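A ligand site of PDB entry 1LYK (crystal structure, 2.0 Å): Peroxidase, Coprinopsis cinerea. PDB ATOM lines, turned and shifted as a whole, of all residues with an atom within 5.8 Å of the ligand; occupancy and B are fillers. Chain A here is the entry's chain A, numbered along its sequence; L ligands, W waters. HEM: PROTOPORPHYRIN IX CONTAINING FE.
Water W4 lies within hydrogen-bond range of O1D of the ligand, NH2 of Arg 47, OG of Ser 44 and OE2 of Glu 189. Water W3 lies within hydrogen-bond range of NH1 of Arg 51 (2.8 Å), O2A of the ligand (2.8 Å) and NZ of Lys 48 (3.0 Å). Water W2 bridges OG of Ser 244 and OD2 of Asp 245. Water W1 lies within hydrogen-bond range of O of Pro 153 (3.0 Å) and NE2 of His 55 (3.2 Å).
Merely in contact with the ligand: Lys 48 (3.6 Å), Leu 50 (3.3 Å), Arg 51 (3.7 Å), Phe 54 (3.5 Å), Pro 153 (3.6 Å), Gly 154 (3.5 Å), Pro 155 (3.7 Å), Ile 162 (3.9 Å), Leu 179 (3.6 Å), Leu 180 (3.6 Å), Ala 182 (3.6 Å), Leu 185 (3.4 Å), Ala 186 (3.4 Å), Gln 188 (3.8 Å), Leu 191 (3.6 Å), Met 242 (3.6 Å), Ser 244 (3.7 Å) and Met 276 (3.8 Å). Hydrophobic or aromatic side chains within 4 Å of the ligand: Leu 50, Phe 54, Pro 155, Ile 162, Leu 179, Leu 180, Ala 182, His 183, Ala 186, Leu 191, Met 242 and Met 276. The nearest printed residue that does not touch the ligand is Tyr 272 (4.01 Å).
NE of Arg 47 is in salt-bridge range of O2D of the ligand. N of Glu 189 lies within hydrogen-bond range of O2A of the ligand (2.9 Å). The backbone NH of Ser 187 sits at hydrogen-bond distance from an oxygen (O2D) of the ligand (3.1 Å). OG of Ser 187 lies within hydrogen-bond range of O2D of the ligand (3.0 Å). The backbone NH (N) of Gly 190 is in hydrogen-bond range of an oxygen (O1A) of the ligand (2.9 Å). An iron atom (FE) of the ligand is bound by a ring nitrogen (NE2) of His 183 (2.3 Å).
The side-chain hydroxyl (OH) of Tyr 272 sits close to the side-chain sulfur (SD) of Met 276, at 3.7 Å. OE1 of Glu 189 is in salt-bridge range of NZ of Lys 48 (2.8 Å). The side-chain sulfur (SD) of Met 242 sits close to the side-chain hydroxyl (OG) of Ser 244. N of Leu 191 lies within hydrogen-bond range of OE1 of Gln 188. The side-chain amide oxygen of Gln 188 lies within hydrogen-bond range of the backbone NH of Gly 190. O of Ala 186 sits at hydrogen-bond distance from N of Leu 200, at 2.9 Å. The side-chain carboxylate of Asp 245 sits at hydrogen-bond distance from a ring nitrogen (ND1) of His 183 (2.9 Å). The backbone NH (N) of Ser 244 sits at hydrogen-bond distance from the backbone carbonyl oxygen (O) of Pro 155.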
ATOM      1  N   SER A  44     -14.125   1.697   6.332  1.00  0.00           N
ATOM      2  CA  SER A  44     -15.212   1.189   5.498  1.00  0.00           C
ATOM      3  C   SER A  44     -14.958   1.228   3.997  1.00  0.00           C
ATOM      4  O   SER A  44     -15.059   0.193   3.330  1.00  0.00           O
ATOM      5  CB  SER A  44     -16.528   1.883   5.839  1.00  0.00           C
ATOM      6  OG  SER A  44     -17.616   1.201   5.239  1.00  0.00           O
ATOM      7  N   VAL A  46     -12.452   0.865   2.113  1.00  0.00           N
ATOM      8  CA  VAL A  46     -11.622  -0.211   1.589  1.00  0.00           C
ATOM      9  C   VAL A  46     -12.389  -1.539   1.566  1.00  0.00           C
ATOM     10  O   VAL A  46     -12.338  -2.278   0.581  1.00  0.00           O
ATOM     11  CB  VAL A  46     -10.332  -0.420   2.429  1.00  0.00           C
ATOM     12  CG1 VAL A  46      -9.519  -1.571   1.867  1.00  0.00           C
ATOM     13  CG2 VAL A  46      -9.491   0.844   2.436  1.00  0.00           C
ATOM     14  N   ARG A  47     -13.120  -1.803   2.642  1.00  0.00           N
ATOM     15  CA  ARG A  47     -13.882  -3.034   2.783  1.00  0.00           C
ATOM     16  C   ARG A  47     -14.974  -3.145   1.722  1.00  0.00           C
ATOM     17  O   ARG A  47     -15.207  -4.205   1.157  1.00  0.00           O
ATOM     18  CB  ARG A  47     -14.475  -3.094   4.176  1.00  0.00           C
ATOM     19  CG  ARG A  47     -13.446  -2.811   5.268  1.00  0.00           C
ATOM     20  CD  ARG A  47     -13.903  -3.282   6.631  1.00  0.00           C
ATOM     21  NE  ARG A  47     -15.109  -2.600   7.094  1.00  0.00           N
ATOM     22  CZ  ARG A  47     -15.108  -1.518   7.869  1.00  0.00           C
ATOM     23  NH1 ARG A  47     -13.954  -0.981   8.246  1.00  0.00           N
ATOM     24  NH2 ARG A  47     -16.250  -1.013   8.290  1.00  0.00           N
ATOM     25  N   LYS A  48     -15.607  -2.002   1.436  1.00  0.00           N
ATOM     26  CA  LYS A  48     -16.647  -1.909   0.429  1.00  0.00           C
ATOM     27  C   LYS A  48     -16.060  -2.170  -0.972  1.00  0.00           C
ATOM     28  O   LYS A  48     -16.630  -2.925  -1.761  1.00  0.00           O
ATOM     29  CB  LYS A  48     -17.248  -0.510   0.470  1.00  0.00           C
ATOM     30  CG  LYS A  48     -17.975  -0.186   1.762  1.00  0.00           C
ATOM     31  CD  LYS A  48     -19.363  -0.762   1.735  1.00  0.00           C
ATOM     32  CE  LYS A  48     -20.083  -0.513   3.044  1.00  0.00           C
ATOM     33  NZ  LYS A  48     -21.474  -1.051   2.980  1.00  0.00           N
ATOM     34  N   LEU A  50     -13.504  -3.795  -1.607  1.00  0.00           N
ATOM     35  CA  LEU A  50     -13.163  -5.211  -1.625  1.00  0.00           C
ATOM     36  C   LEU A  50     -14.387  -6.082  -1.942  1.00  0.00           C
ATOM     37  O   LEU A  50     -14.257  -7.146  -2.532  1.00  0.00           O
ATOM     38  CB  LEU A  50     -12.515  -5.642  -0.303  1.00  0.00           C
ATOM     39  CG  LEU A  50     -10.998  -5.550  -0.282  1.00  0.00           C
ATOM     40  CD1 LEU A  50     -10.487  -5.872   1.100  1.00  0.00           C
ATOM     41  CD2 LEU A  50     -10.406  -6.482  -1.318  1.00  0.00           C
ATOM     42  N   ARG A  51     -15.569  -5.632  -1.521  1.00  0.00           N
ATOM     43  CA  ARG A  51     -16.791  -6.365  -1.826  1.00  0.00           C
ATOM     44  C   ARG A  51     -17.095  -6.179  -3.298  1.00  0.00           C
ATOM     45  O   ARG A  51     -17.459  -7.133  -4.004  1.00  0.00           O
ATOM     46  CB  ARG A  51     -17.953  -5.828  -1.010  1.00  0.00           C
ATOM     47  CG  ARG A  51     -18.299  -6.663   0.161  1.00  0.00           C
ATOM     48  CD  ARG A  51     -19.489  -6.093   0.872  1.00  0.00           C
ATOM     49  NE  ARG A  51     -20.735  -6.526   0.264  1.00  0.00           N
ATOM     50  CZ  ARG A  51     -21.846  -5.800   0.268  1.00  0.00           C
ATOM     51  NH1 ARG A  51     -21.862  -4.598   0.833  1.00  0.00           N
ATOM     52  NH2 ARG A  51     -22.966  -6.314  -0.203  1.00  0.00           N
ATOM     53  N   VAL A  53     -14.993  -5.393  -5.879  1.00  0.00           N
ATOM     54  CA  VAL A  53     -14.079  -6.079  -6.794  1.00  0.00           C
ATOM     55  C   VAL A  53     -14.438  -7.547  -6.948  1.00  0.00           C
ATOM     56  O   VAL A  53     -14.365  -8.098  -8.063  1.00  0.00           O
ATOM     57  CB  VAL A  53     -12.593  -5.899  -6.407  1.00  0.00           C
ATOM     58  CG1 VAL A  53     -12.254  -6.626  -5.106  1.00  0.00           C
ATOM     59  CG2 VAL A  53     -11.700  -6.353  -7.546  1.00  0.00           C
ATOM     60  N   PHE A  54     -14.869  -8.173  -5.856  1.00  0.00           N
ATOM     61  CA  PHE A  54     -15.271  -9.565  -5.904  1.00  0.00           C
ATOM     62  C   PHE A  54     -16.601  -9.684  -6.665  1.00  0.00           C
ATOM     63  O   PHE A  54     -16.730 -10.515  -7.557  1.00  0.00           O
ATOM     64  CB  PHE A  54     -15.407 -10.134  -4.479  1.00  0.00           C
ATOM     65  CG  PHE A  54     -16.016 -11.515  -4.425  1.00  0.00           C
ATOM     66  CD1 PHE A  54     -17.035 -11.813  -3.509  1.00  0.00           C
ATOM     67  CD2 PHE A  54     -15.612 -12.502  -5.300  1.00  0.00           C
ATOM     68  CE1 PHE A  54     -17.627 -13.074  -3.465  1.00  0.00           C
ATOM     69  CE2 PHE A  54     -16.181 -13.769  -5.270  1.00  0.00           C
ATOM     70  CZ  PHE A  54     -17.204 -14.058  -4.351  1.00  0.00           C
ATOM     71  N   HIS A  55     -17.570  -8.829  -6.335  1.00  0.00           N
ATOM     72  CA  HIS A  55     -18.877  -8.898  -6.996  1.00  0.00           C
ATOM     73  C   HIS A  55     -18.810  -8.500  -8.459  1.00  0.00           C
ATOM     74  O   HIS A  55     -19.630  -8.943  -9.254  1.00  0.00           O
ATOM     75  CB  HIS A  55     -19.911  -8.072  -6.233  1.00  0.00           C
ATOM     76  CG  HIS A  55     -20.239  -8.623  -4.873  1.00  0.00           C
ATOM     77  ND1 HIS A  55     -21.317  -8.203  -4.134  1.00  0.00           N
ATOM     78  CD2 HIS A  55     -19.625  -9.582  -4.131  1.00  0.00           C
ATOM     79  CE1 HIS A  55     -21.359  -8.865  -2.995  1.00  0.00           C
ATOM     80  NE2 HIS A  55     -20.346  -9.712  -2.968  1.00  0.00           N
ATOM     81  N   PRO A 153     -21.830 -15.852  -4.904  1.00  0.00           N
ATOM     82  CA  PRO A 153     -22.117 -16.768  -3.781  1.00  0.00           C
ATOM     83  C   PRO A 153     -22.681 -16.002  -2.581  1.00  0.00           C
ATOM     84  O   PRO A 153     -22.273 -14.874  -2.306  1.00  0.00           O
ATOM     85  CB  PRO A 153     -20.743 -17.340  -3.464  1.00  0.00           C
ATOM     86  CG  PRO A 153     -20.076 -17.390  -4.824  1.00  0.00           C
ATOM     87  CD  PRO A 153     -20.438 -16.021  -5.379  1.00  0.00           C
ATOM     88  N   GLY A 154     -23.647 -16.596  -1.884  1.00  0.00           N
ATOM     89  CA  GLY A 154     -24.256 -15.941  -0.725  1.00  0.00           C
ATOM     90  C   GLY A 154     -23.894 -16.652   0.566  1.00  0.00           C
ATOM     91  O   GLY A 154     -23.555 -17.840   0.543  1.00  0.00           O
ATOM     92  N   PRO A 155     -24.020 -15.992   1.728  1.00  0.00           N
ATOM     93  CA  PRO A 155     -23.685 -16.586   3.020  1.00  0.00           C
ATOM     94  C   PRO A 155     -24.471 -17.833   3.470  1.00  0.00           C
ATOM     95  O   PRO A 155     -23.998 -18.586   4.325  1.00  0.00           O
ATOM     96  CB  PRO A 155     -23.838 -15.407   3.977  1.00  0.00           C
ATOM     97  CG  PRO A 155     -24.931 -14.627   3.359  1.00  0.00           C
ATOM     98  CD  PRO A 155     -24.550 -14.638   1.896  1.00  0.00           C
ATOM     99  N   ILE A 162     -21.142 -23.223  -3.285  1.00  0.00           N
ATOM    100  CA  ILE A 162     -20.066 -22.251  -3.308  1.00  0.00           C
ATOM    101  C   ILE A 162     -18.888 -22.719  -4.156  1.00  0.00           C
ATOM    102  O   ILE A 162     -18.417 -21.977  -5.030  1.00  0.00           O
ATOM    103  CB  ILE A 162     -19.606 -21.915  -1.876  1.00  0.00           C
ATOM    104  CG1 ILE A 162     -20.708 -21.120  -1.173  1.00  0.00           C
ATOM    105  CG2 ILE A 162     -18.292 -21.119  -1.886  1.00  0.00           C
ATOM    106  CD1 ILE A 162     -20.418 -20.809   0.266  1.00  0.00           C
ATOM    107  N   MET A 166     -17.724 -21.038  -7.775  1.00  0.00           N
ATOM    108  CA  MET A 166     -16.344 -20.581  -7.892  1.00  0.00           C
ATOM    109  C   MET A 166     -15.562 -21.442  -8.881  1.00  0.00           C
ATOM    110  O   MET A 166     -14.729 -20.928  -9.624  1.00  0.00           O
ATOM    111  CB  MET A 166     -15.657 -20.599  -6.518  1.00  0.00           C
ATOM    112  CG  MET A 166     -16.282 -19.658  -5.485  1.00  0.00           C
ATOM    113  SD  MET A 166     -16.256 -17.909  -5.907  1.00  0.00           S
ATOM    114  CE  MET A 166     -14.542 -17.477  -5.461  1.00  0.00           C
ATOM    115  N   VAL A 176     -10.456 -20.783  -3.318  1.00  0.00           N
ATOM    116  CA  VAL A 176     -11.630 -20.202  -2.671  1.00  0.00           C
ATOM    117  C   VAL A 176     -11.221 -19.792  -1.245  1.00  0.00           C
ATOM    118  O   VAL A 176     -11.524 -18.684  -0.783  1.00  0.00           O
ATOM    119  CB  VAL A 176     -12.811 -21.182  -2.639  1.00  0.00           C
ATOM    120  CG1 VAL A 176     -14.007 -20.521  -1.978  1.00  0.00           C
ATOM    121  CG2 VAL A 176     -13.174 -21.634  -4.052  1.00  0.00           C
ATOM    122  N   LEU A 179      -8.900 -16.664  -1.486  1.00  0.00           N
ATOM    123  CA  LEU A 179      -9.640 -15.425  -1.754  1.00  0.00           C
ATOM    124  C   LEU A 179     -10.306 -14.890  -0.494  1.00  0.00           C
ATOM    125  O   LEU A 179     -10.405 -13.670  -0.307  1.00  0.00           O
ATOM    126  CB  LEU A 179     -10.710 -15.653  -2.825  1.00  0.00           C
ATOM    127  CG  LEU A 179     -10.528 -15.286  -4.310  1.00  0.00           C
ATOM    128  CD1 LEU A 179      -9.398 -14.309  -4.557  1.00  0.00           C
ATOM    129  CD2 LEU A 179     -10.339 -16.537  -5.115  1.00  0.00           C
ATOM    130  N   LEU A 180     -10.770 -15.787   0.362  1.00  0.00           N
ATOM    131  CA  LEU A 180     -11.445 -15.402   1.601  1.00  0.00           C
ATOM    132  C   LEU A 180     -10.588 -14.704   2.674  1.00  0.00           C
ATOM    133  O   LEU A 180     -11.094 -14.340   3.737  1.00  0.00           O
ATOM    134  CB  LEU A 180     -12.168 -16.604   2.210  1.00  0.00           C
ATOM    135  CG  LEU A 180     -13.547 -16.875   1.633  1.00  0.00           C
ATOM    136  CD1 LEU A 180     -14.002 -18.249   2.031  1.00  0.00           C
ATOM    137  CD2 LEU A 180     -14.506 -15.814   2.132  1.00  0.00           C
ATOM    138  N   ALA A 182      -9.660 -11.889   2.478  1.00  0.00           N
ATOM    139  CA  ALA A 182     -10.216 -10.532   2.499  1.00  0.00           C
ATOM    140  C   ALA A 182     -11.132 -10.314   3.690  1.00  0.00           C
ATOM    141  O   ALA A 182     -11.345  -9.179   4.108  1.00  0.00           O
ATOM    142  CB  ALA A 182     -10.961 -10.242   1.204  1.00  0.00           C
ATOM    143  N   HIS A 183     -11.690 -11.398   4.241  1.00  0.00           N
ATOM    144  CA  HIS A 183     -12.559 -11.281   5.413  1.00  0.00           C
ATOM    145  C   HIS A 183     -11.791 -10.894   6.687  1.00  0.00           C
ATOM    146  O   HIS A 183     -12.380 -10.675   7.747  1.00  0.00           O
ATOM    147  CB  HIS A 183     -13.397 -12.537   5.637  1.00  0.00           C
ATOM    148  CG  HIS A 183     -14.646 -12.602   4.760  1.00  0.00           C
ATOM    149  ND1 HIS A 183     -15.720 -13.489   4.889  1.00  0.00           N
ATOM    150  CD2 HIS A 183     -14.898 -11.765   3.686  1.00  0.00           C
ATOM    151  CE1 HIS A 183     -16.555 -13.241   3.889  1.00  0.00           C
ATOM    152  NE2 HIS A 183     -16.111 -12.225   3.204  1.00  0.00           N
ATOM    153  N   LEU A 185     -10.336  -8.160   6.881  1.00  0.00           N
ATOM    154  CA  LEU A 185     -10.541  -6.710   6.912  1.00  0.00           C
ATOM    155  C   LEU A 185     -12.036  -6.567   6.597  1.00  0.00           C
ATOM    156  O   LEU A 185     -12.413  -5.953   5.597  1.00  0.00           O
ATOM    157  CB  LEU A 185      -9.725  -6.050   5.790  1.00  0.00           C
ATOM    158  CG  LEU A 185      -8.199  -6.149   5.739  1.00  0.00           C
ATOM    159  CD1 LEU A 185      -7.683  -5.650   4.406  1.00  0.00           C
ATOM    160  CD2 LEU A 185      -7.608  -5.327   6.862  1.00  0.00           C
ATOM    161  N   ALA A 186     -12.884  -7.080   7.486  1.00  0.00           N
ATOM    162  CA  ALA A 186     -14.314  -7.080   7.215  1.00  0.00           C
ATOM    163  C   ALA A 186     -15.261  -6.978   8.391  1.00  0.00           C
ATOM    164  O   ALA A 186     -14.918  -7.321   9.527  1.00  0.00           O
ATOM    165  CB  ALA A 186     -14.665  -8.328   6.404  1.00  0.00           C
ATOM    166  N   SER A 187     -16.479  -6.531   8.095  1.00  0.00           N
ATOM    167  CA  SER A 187     -17.554  -6.403   9.069  1.00  0.00           C
ATOM    168  C   SER A 187     -18.821  -6.707   8.253  1.00  0.00           C
ATOM    169  O   SER A 187     -18.732  -6.974   7.053  1.00  0.00           O
ATOM    170  CB  SER A 187     -17.646  -4.981   9.621  1.00  0.00           C
ATOM    171  OG  SER A 187     -18.267  -4.090   8.697  1.00  0.00           O
ATOM    172  N   GLN A 188     -19.972  -6.749   8.905  1.00  0.00           N
ATOM    173  CA  GLN A 188     -21.214  -6.974   8.182  1.00  0.00           C
ATOM    174  C   GLN A 188     -22.124  -5.821   8.578  1.00  0.00           C
ATOM    175  O   GLN A 188     -22.030  -5.294   9.689  1.00  0.00           O
ATOM    176  CB  GLN A 188     -21.845  -8.327   8.529  1.00  0.00           C
ATOM    177  CG  GLN A 188     -22.350  -8.493   9.960  1.00  0.00           C
ATOM    178  CD  GLN A 188     -23.651  -7.743  10.245  1.00  0.00           C
ATOM    179  OE1 GLN A 188     -24.529  -7.640   9.393  1.00  0.00           O
ATOM    180  NE2 GLN A 188     -23.748  -7.202  11.440  1.00  0.00           N
ATOM    181  N   GLU A 189     -22.971  -5.373   7.654  1.00  0.00           N
ATOM    182  CA  GLU A 189     -23.895  -4.280   7.955  1.00  0.00           C
ATOM    183  C   GLU A 189     -25.325  -4.720   7.653  1.00  0.00           C
ATOM    184  O   GLU A 189     -26.269  -4.225   8.286  1.00  0.00           O
ATOM    185  CB  GLU A 189     -23.565  -3.038   7.118  1.00  0.00           C
ATOM    186  CG  GLU A 189     -22.174  -2.452   7.317  1.00  0.00           C
ATOM    187  CD  GLU A 189     -21.943  -1.225   6.462  1.00  0.00           C
ATOM    188  OE1 GLU A 189     -22.736  -0.998   5.528  1.00  0.00           O
ATOM    189  OE2 GLU A 189     -20.991  -0.490   6.707  1.00  0.00           O
ATOM    190  N   GLY A 190     -25.482  -5.660   6.734  1.00  0.00           N
ATOM    191  CA  GLY A 190     -26.803  -6.107   6.348  1.00  0.00           C
ATOM    192  C   GLY A 190     -27.317  -7.465   6.781  1.00  0.00           C
ATOM    193  O   GLY A 190     -28.458  -7.794   6.491  1.00  0.00           O
ATOM    194  N   LEU A 191     -26.491  -8.275   7.446  1.00  0.00           N
ATOM    195  CA  LEU A 191     -26.986  -9.587   7.877  1.00  0.00           C
ATOM    196  C   LEU A 191     -27.709  -9.463   9.223  1.00  0.00           C
ATOM    197  O   LEU A 191     -28.694 -10.164   9.463  1.00  0.00           O
ATOM    198  CB  LEU A 191     -25.868 -10.639   7.915  1.00  0.00           C
ATOM    199  CG  LEU A 191     -25.145 -10.925   6.586  1.00  0.00           C
ATOM    200  CD1 LEU A 191     -24.144 -12.043   6.756  1.00  0.00           C
ATOM    201  CD2 LEU A 191     -26.145 -11.296   5.510  1.00  0.00           C
ATOM    202  N   LEU A 200     -15.539  -9.347  11.478  1.00  0.00           N
ATOM    203  CA  LEU A 200     -15.479 -10.773  11.173  1.00  0.00           C
ATOM    204  C   LEU A 200     -14.246 -11.388  11.870  1.00  0.00           C
ATOM    205  O   LEU A 200     -14.140 -12.609  11.967  1.00  0.00           O
ATOM    206  CB  LEU A 200     -15.469 -10.988   9.657  1.00  0.00           C
ATOM    207  CG  LEU A 200     -16.788 -11.369   8.959  1.00  0.00           C
ATOM    208  CD1 LEU A 200     -17.973 -10.530   9.415  1.00  0.00           C
ATOM    209  CD2 LEU A 200     -16.605 -11.259   7.463  1.00  0.00           C
ATOM    210  N   MET A 242     -20.218 -15.559  10.020  1.00  0.00           N
ATOM    211  CA  MET A 242     -21.060 -15.826   8.853  1.00  0.00           C
ATOM    212  C   MET A 242     -21.133 -17.343   8.663  1.00  0.00           C
ATOM    213  O   MET A 242     -20.121 -18.030   8.788  1.00  0.00           O
ATOM    214  CB  MET A 242     -20.366 -15.182   7.657  1.00  0.00           C
ATOM    215  CG  MET A 242     -21.243 -14.939   6.460  1.00  0.00           C
ATOM    216  SD  MET A 242     -20.290 -14.086   5.182  1.00  0.00           S
ATOM    217  CE  MET A 242     -19.747 -12.696   6.098  1.00  0.00           C
ATOM    218  N   SER A 244     -21.366 -19.318   5.934  1.00  0.00           N
ATOM    219  CA  SER A 244     -20.493 -19.866   4.904  1.00  0.00           C
ATOM    220  C   SER A 244     -19.031 -19.960   5.372  1.00  0.00           C
ATOM    221  O   SER A 244     -18.316 -20.921   5.057  1.00  0.00           O
ATOM    222  CB  SER A 244     -20.599 -19.028   3.635  1.00  0.00           C
ATOM    223  OG  SER A 244     -20.498 -17.647   3.948  1.00  0.00           O
ATOM    224  N   ASP A 245     -18.571 -18.968   6.124  1.00  0.00           N
ATOM    225  CA  ASP A 245     -17.198 -19.001   6.628  1.00  0.00           C
ATOM    226  C   ASP A 245     -17.050 -20.160   7.611  1.00  0.00           C
ATOM    227  O   ASP A 245     -16.089 -20.924   7.555  1.00  0.00           O
ATOM    228  CB  ASP A 245     -16.836 -17.694   7.316  1.00  0.00           C
ATOM    229  CG  ASP A 245     -16.631 -16.560   6.344  1.00  0.00           C
ATOM    230  OD1 ASP A 245     -16.738 -15.389   6.767  1.00  0.00           O
ATOM    231  OD2 ASP A 245     -16.339 -16.833   5.159  1.00  0.00           O
ATOM    232  N   LEU A 248     -17.046 -23.467   5.650  1.00  0.00           N
ATOM    233  CA  LEU A 248     -15.841 -23.606   4.845  1.00  0.00           C
ATOM    234  C   LEU A 248     -14.658 -23.985   5.736  1.00  0.00           C
ATOM    235  O   LEU A 248     -13.867 -24.841   5.376  1.00  0.00           O
ATOM    236  CB  LEU A 248     -15.566 -22.334   4.043  1.00  0.00           C
ATOM    237  CG  LEU A 248     -16.484 -22.138   2.825  1.00  0.00           C
ATOM    238  CD1 LEU A 248     -16.299 -20.759   2.252  1.00  0.00           C
ATOM    239  CD2 LEU A 248     -16.198 -23.182   1.763  1.00  0.00           C
ATOM    240  N   TYR A 272      -3.235 -15.186  -1.299  1.00  0.00           N
ATOM    241  CA  TYR A 272      -4.291 -14.233  -1.618  1.00  0.00           C
ATOM    242  C   TYR A 272      -3.895 -13.395  -2.849  1.00  0.00           C
ATOM    243  O   TYR A 272      -4.674 -13.273  -3.798  1.00  0.00           O
ATOM    244  CB  TYR A 272      -4.537 -13.327  -0.440  1.00  0.00           C
ATOM    245  CG  TYR A 272      -5.510 -12.200  -0.681  1.00  0.00           C
ATOM    246  CD1 TYR A 272      -5.056 -10.884  -0.813  1.00  0.00           C
ATOM    247  CD2 TYR A 272      -6.884 -12.441  -0.749  1.00  0.00           C
ATOM    248  CE1 TYR A 272      -5.941  -9.842  -0.979  1.00  0.00           C
ATOM    249  CE2 TYR A 272      -7.780 -11.396  -0.909  1.00  0.00           C
ATOM    250  CZ  TYR A 272      -7.300 -10.110  -1.025  1.00  0.00           C
ATOM    251  OH  TYR A 272      -8.169  -9.059  -1.141  1.00  0.00           O
ATOM    252  N   MET A 276      -5.984 -13.233  -6.211  1.00  0.00           N
ATOM    253  CA  MET A 276      -6.493 -11.944  -6.665  1.00  0.00           C
ATOM    254  C   MET A 276      -6.040 -11.594  -8.082  1.00  0.00           C
ATOM    255  O   MET A 276      -6.823 -11.036  -8.860  1.00  0.00           O
ATOM    256  CB  MET A 276      -6.104 -10.834  -5.715  1.00  0.00           C
ATOM    257  CG  MET A 276      -6.845 -10.866  -4.386  1.00  0.00           C
ATOM    258  SD  MET A 276      -8.625 -10.582  -4.521  1.00  0.00           S
ATOM    259  CE  MET A 276      -8.641  -8.789  -4.763  1.00  0.00           C
ATOM    260  N   MET A 279      -8.239 -13.455 -10.356  1.00  0.00           N
ATOM    261  CA  MET A 279      -9.572 -12.893 -10.385  1.00  0.00           C
ATOM    262  C   MET A 279      -9.618 -11.556 -11.117  1.00  0.00           C
ATOM    263  O   MET A 279     -10.643 -11.185 -11.681  1.00  0.00           O
ATOM    264  CB  MET A 279     -10.116 -12.704  -8.964  1.00  0.00           C
ATOM    265  CG  MET A 279     -11.531 -12.180  -8.944  1.00  0.00           C
ATOM    266  SD  MET A 279     -12.295 -12.175  -7.343  1.00  0.00           S
ATOM    267  CE  MET A 279     -11.721 -10.646  -6.765  1.00  0.00           C
HETATM  268  CHA HEM L   1     -18.517  -8.889   3.643  1.00  0.00           C
HETATM  269  CHB HEM L   1     -20.276 -13.017   1.770  1.00  0.00           C
HETATM  270  CHC HEM L   1     -16.058 -13.832  -0.432  1.00  0.00           C
HETATM  271  CHD HEM L   1     -14.682  -9.301   0.695  1.00  0.00           C
HETATM  272  C1A HEM L   1     -19.361  -9.939   3.308  1.00  0.00           C
HETATM  273  C2A HEM L   1     -20.744 -10.019   3.653  1.00  0.00           C
HETATM  274  C3A HEM L   1     -21.248 -11.061   3.077  1.00  0.00           C
HETATM  275  C4A HEM L   1     -20.159 -11.743   2.401  1.00  0.00           C
HETATM  276  CMA HEM L   1     -22.724 -11.446   3.143  1.00  0.00           C
HETATM  277  CAA HEM L   1     -21.518  -9.107   4.589  1.00  0.00           C
HETATM  278  CBA HEM L   1     -21.885  -7.843   3.858  1.00  0.00           C
HETATM  279  CGA HEM L   1     -22.748  -6.948   4.679  1.00  0.00           C
HETATM  280  O1A HEM L   1     -23.770  -7.419   5.197  1.00  0.00           O
HETATM  281  O2A HEM L   1     -22.399  -5.757   4.824  1.00  0.00           O
HETATM  282  C1B HEM L   1     -19.246 -13.697   1.080  1.00  0.00           C
HETATM  283  C2B HEM L   1     -19.286 -15.030   0.535  1.00  0.00           C
HETATM  284  C3B HEM L   1     -18.083 -15.217  -0.081  1.00  0.00           C
HETATM  285  C4B HEM L   1     -17.300 -14.044   0.124  1.00  0.00           C
HETATM  286  CMB HEM L   1     -20.444 -16.039   0.607  1.00  0.00           C
HETATM  287  CAB HEM L   1     -17.648 -16.301  -0.887  1.00  0.00           C
HETATM  288  CBB HEM L   1     -17.533 -17.629  -0.399  1.00  0.00           C
HETATM  289  C1C HEM L   1     -15.291 -12.652  -0.343  1.00  0.00           C
HETATM  290  C2C HEM L   1     -14.190 -12.348  -1.267  1.00  0.00           C
HETATM  291  C3C HEM L   1     -13.894 -11.018  -1.058  1.00  0.00           C
HETATM  292  C4C HEM L   1     -14.715 -10.584   0.097  1.00  0.00           C
HETATM  293  CMC HEM L   1     -13.515 -13.371  -2.193  1.00  0.00           C
HETATM  294  CAC HEM L   1     -13.058 -10.182  -1.826  1.00  0.00           C
HETATM  295  CBC HEM L   1     -11.709 -10.545  -2.288  1.00  0.00           C
HETATM  296  C1D HEM L   1     -15.572  -8.798   1.646  1.00  0.00           C
HETATM  297  C2D HEM L   1     -15.322  -7.634   2.508  1.00  0.00           C
HETATM  298  C3D HEM L   1     -16.390  -7.556   3.331  1.00  0.00           C
HETATM  299  C4D HEM L   1     -17.264  -8.672   3.058  1.00  0.00           C
HETATM  300  CMD HEM L   1     -14.034  -6.851   2.716  1.00  0.00           C
HETATM  301  CAD HEM L   1     -16.581  -6.492   4.346  1.00  0.00           C
HETATM  302  CBD HEM L   1     -17.496  -5.390   3.873  1.00  0.00           C
HETATM  303  CGD HEM L   1     -17.652  -4.270   4.878  1.00  0.00           C
HETATM  304  O1D HEM L   1     -18.332  -3.282   4.568  1.00  0.00           O
HETATM  305  O2D HEM L   1     -17.087  -4.388   5.990  1.00  0.00           O
HETATM  306  NA  HEM L   1     -19.010 -11.008   2.539  1.00  0.00           N
HETATM  307  NB  HEM L   1     -18.002 -13.119   0.863  1.00  0.00           N
HETATM  308  NC  HEM L   1     -15.565 -11.590   0.475  1.00  0.00           N
HETATM  309  ND  HEM L   1     -16.745  -9.451   2.030  1.00  0.00           N
HETATM  310 FE   HEM L   1     -17.403 -11.333   1.483  1.00  0.00          FE
HETATM  311  O   HOH W   1     -21.635 -12.125  -1.308  1.00  0.00           O
HETATM  312  O   HOH W   2     -18.089 -17.051   2.986  1.00  0.00           O
HETATM  313  O   HOH W   3     -20.783  -3.982   3.348  1.00  0.00           O
HETATM  314  O   HOH W   4     -18.261  -1.255   6.427  1.00  0.00           O
HETATM  315  O   HOH W   5     -24.408  -4.068   3.274  1.00  0.00           O
HETATM  316  O   HOH W   6     -24.053 -11.988   0.098  1.00  0.00           O
HETATM  317  O   HOH W   7     -24.111  -9.371   0.932  1.00  0.00           O
HETATM  318  O   HOH W   8     -18.828 -10.161  -0.589  1.00  0.00           O
HETATM  319  O   HOH W   9     -25.455  -8.664   3.477  1.00  0.00           O
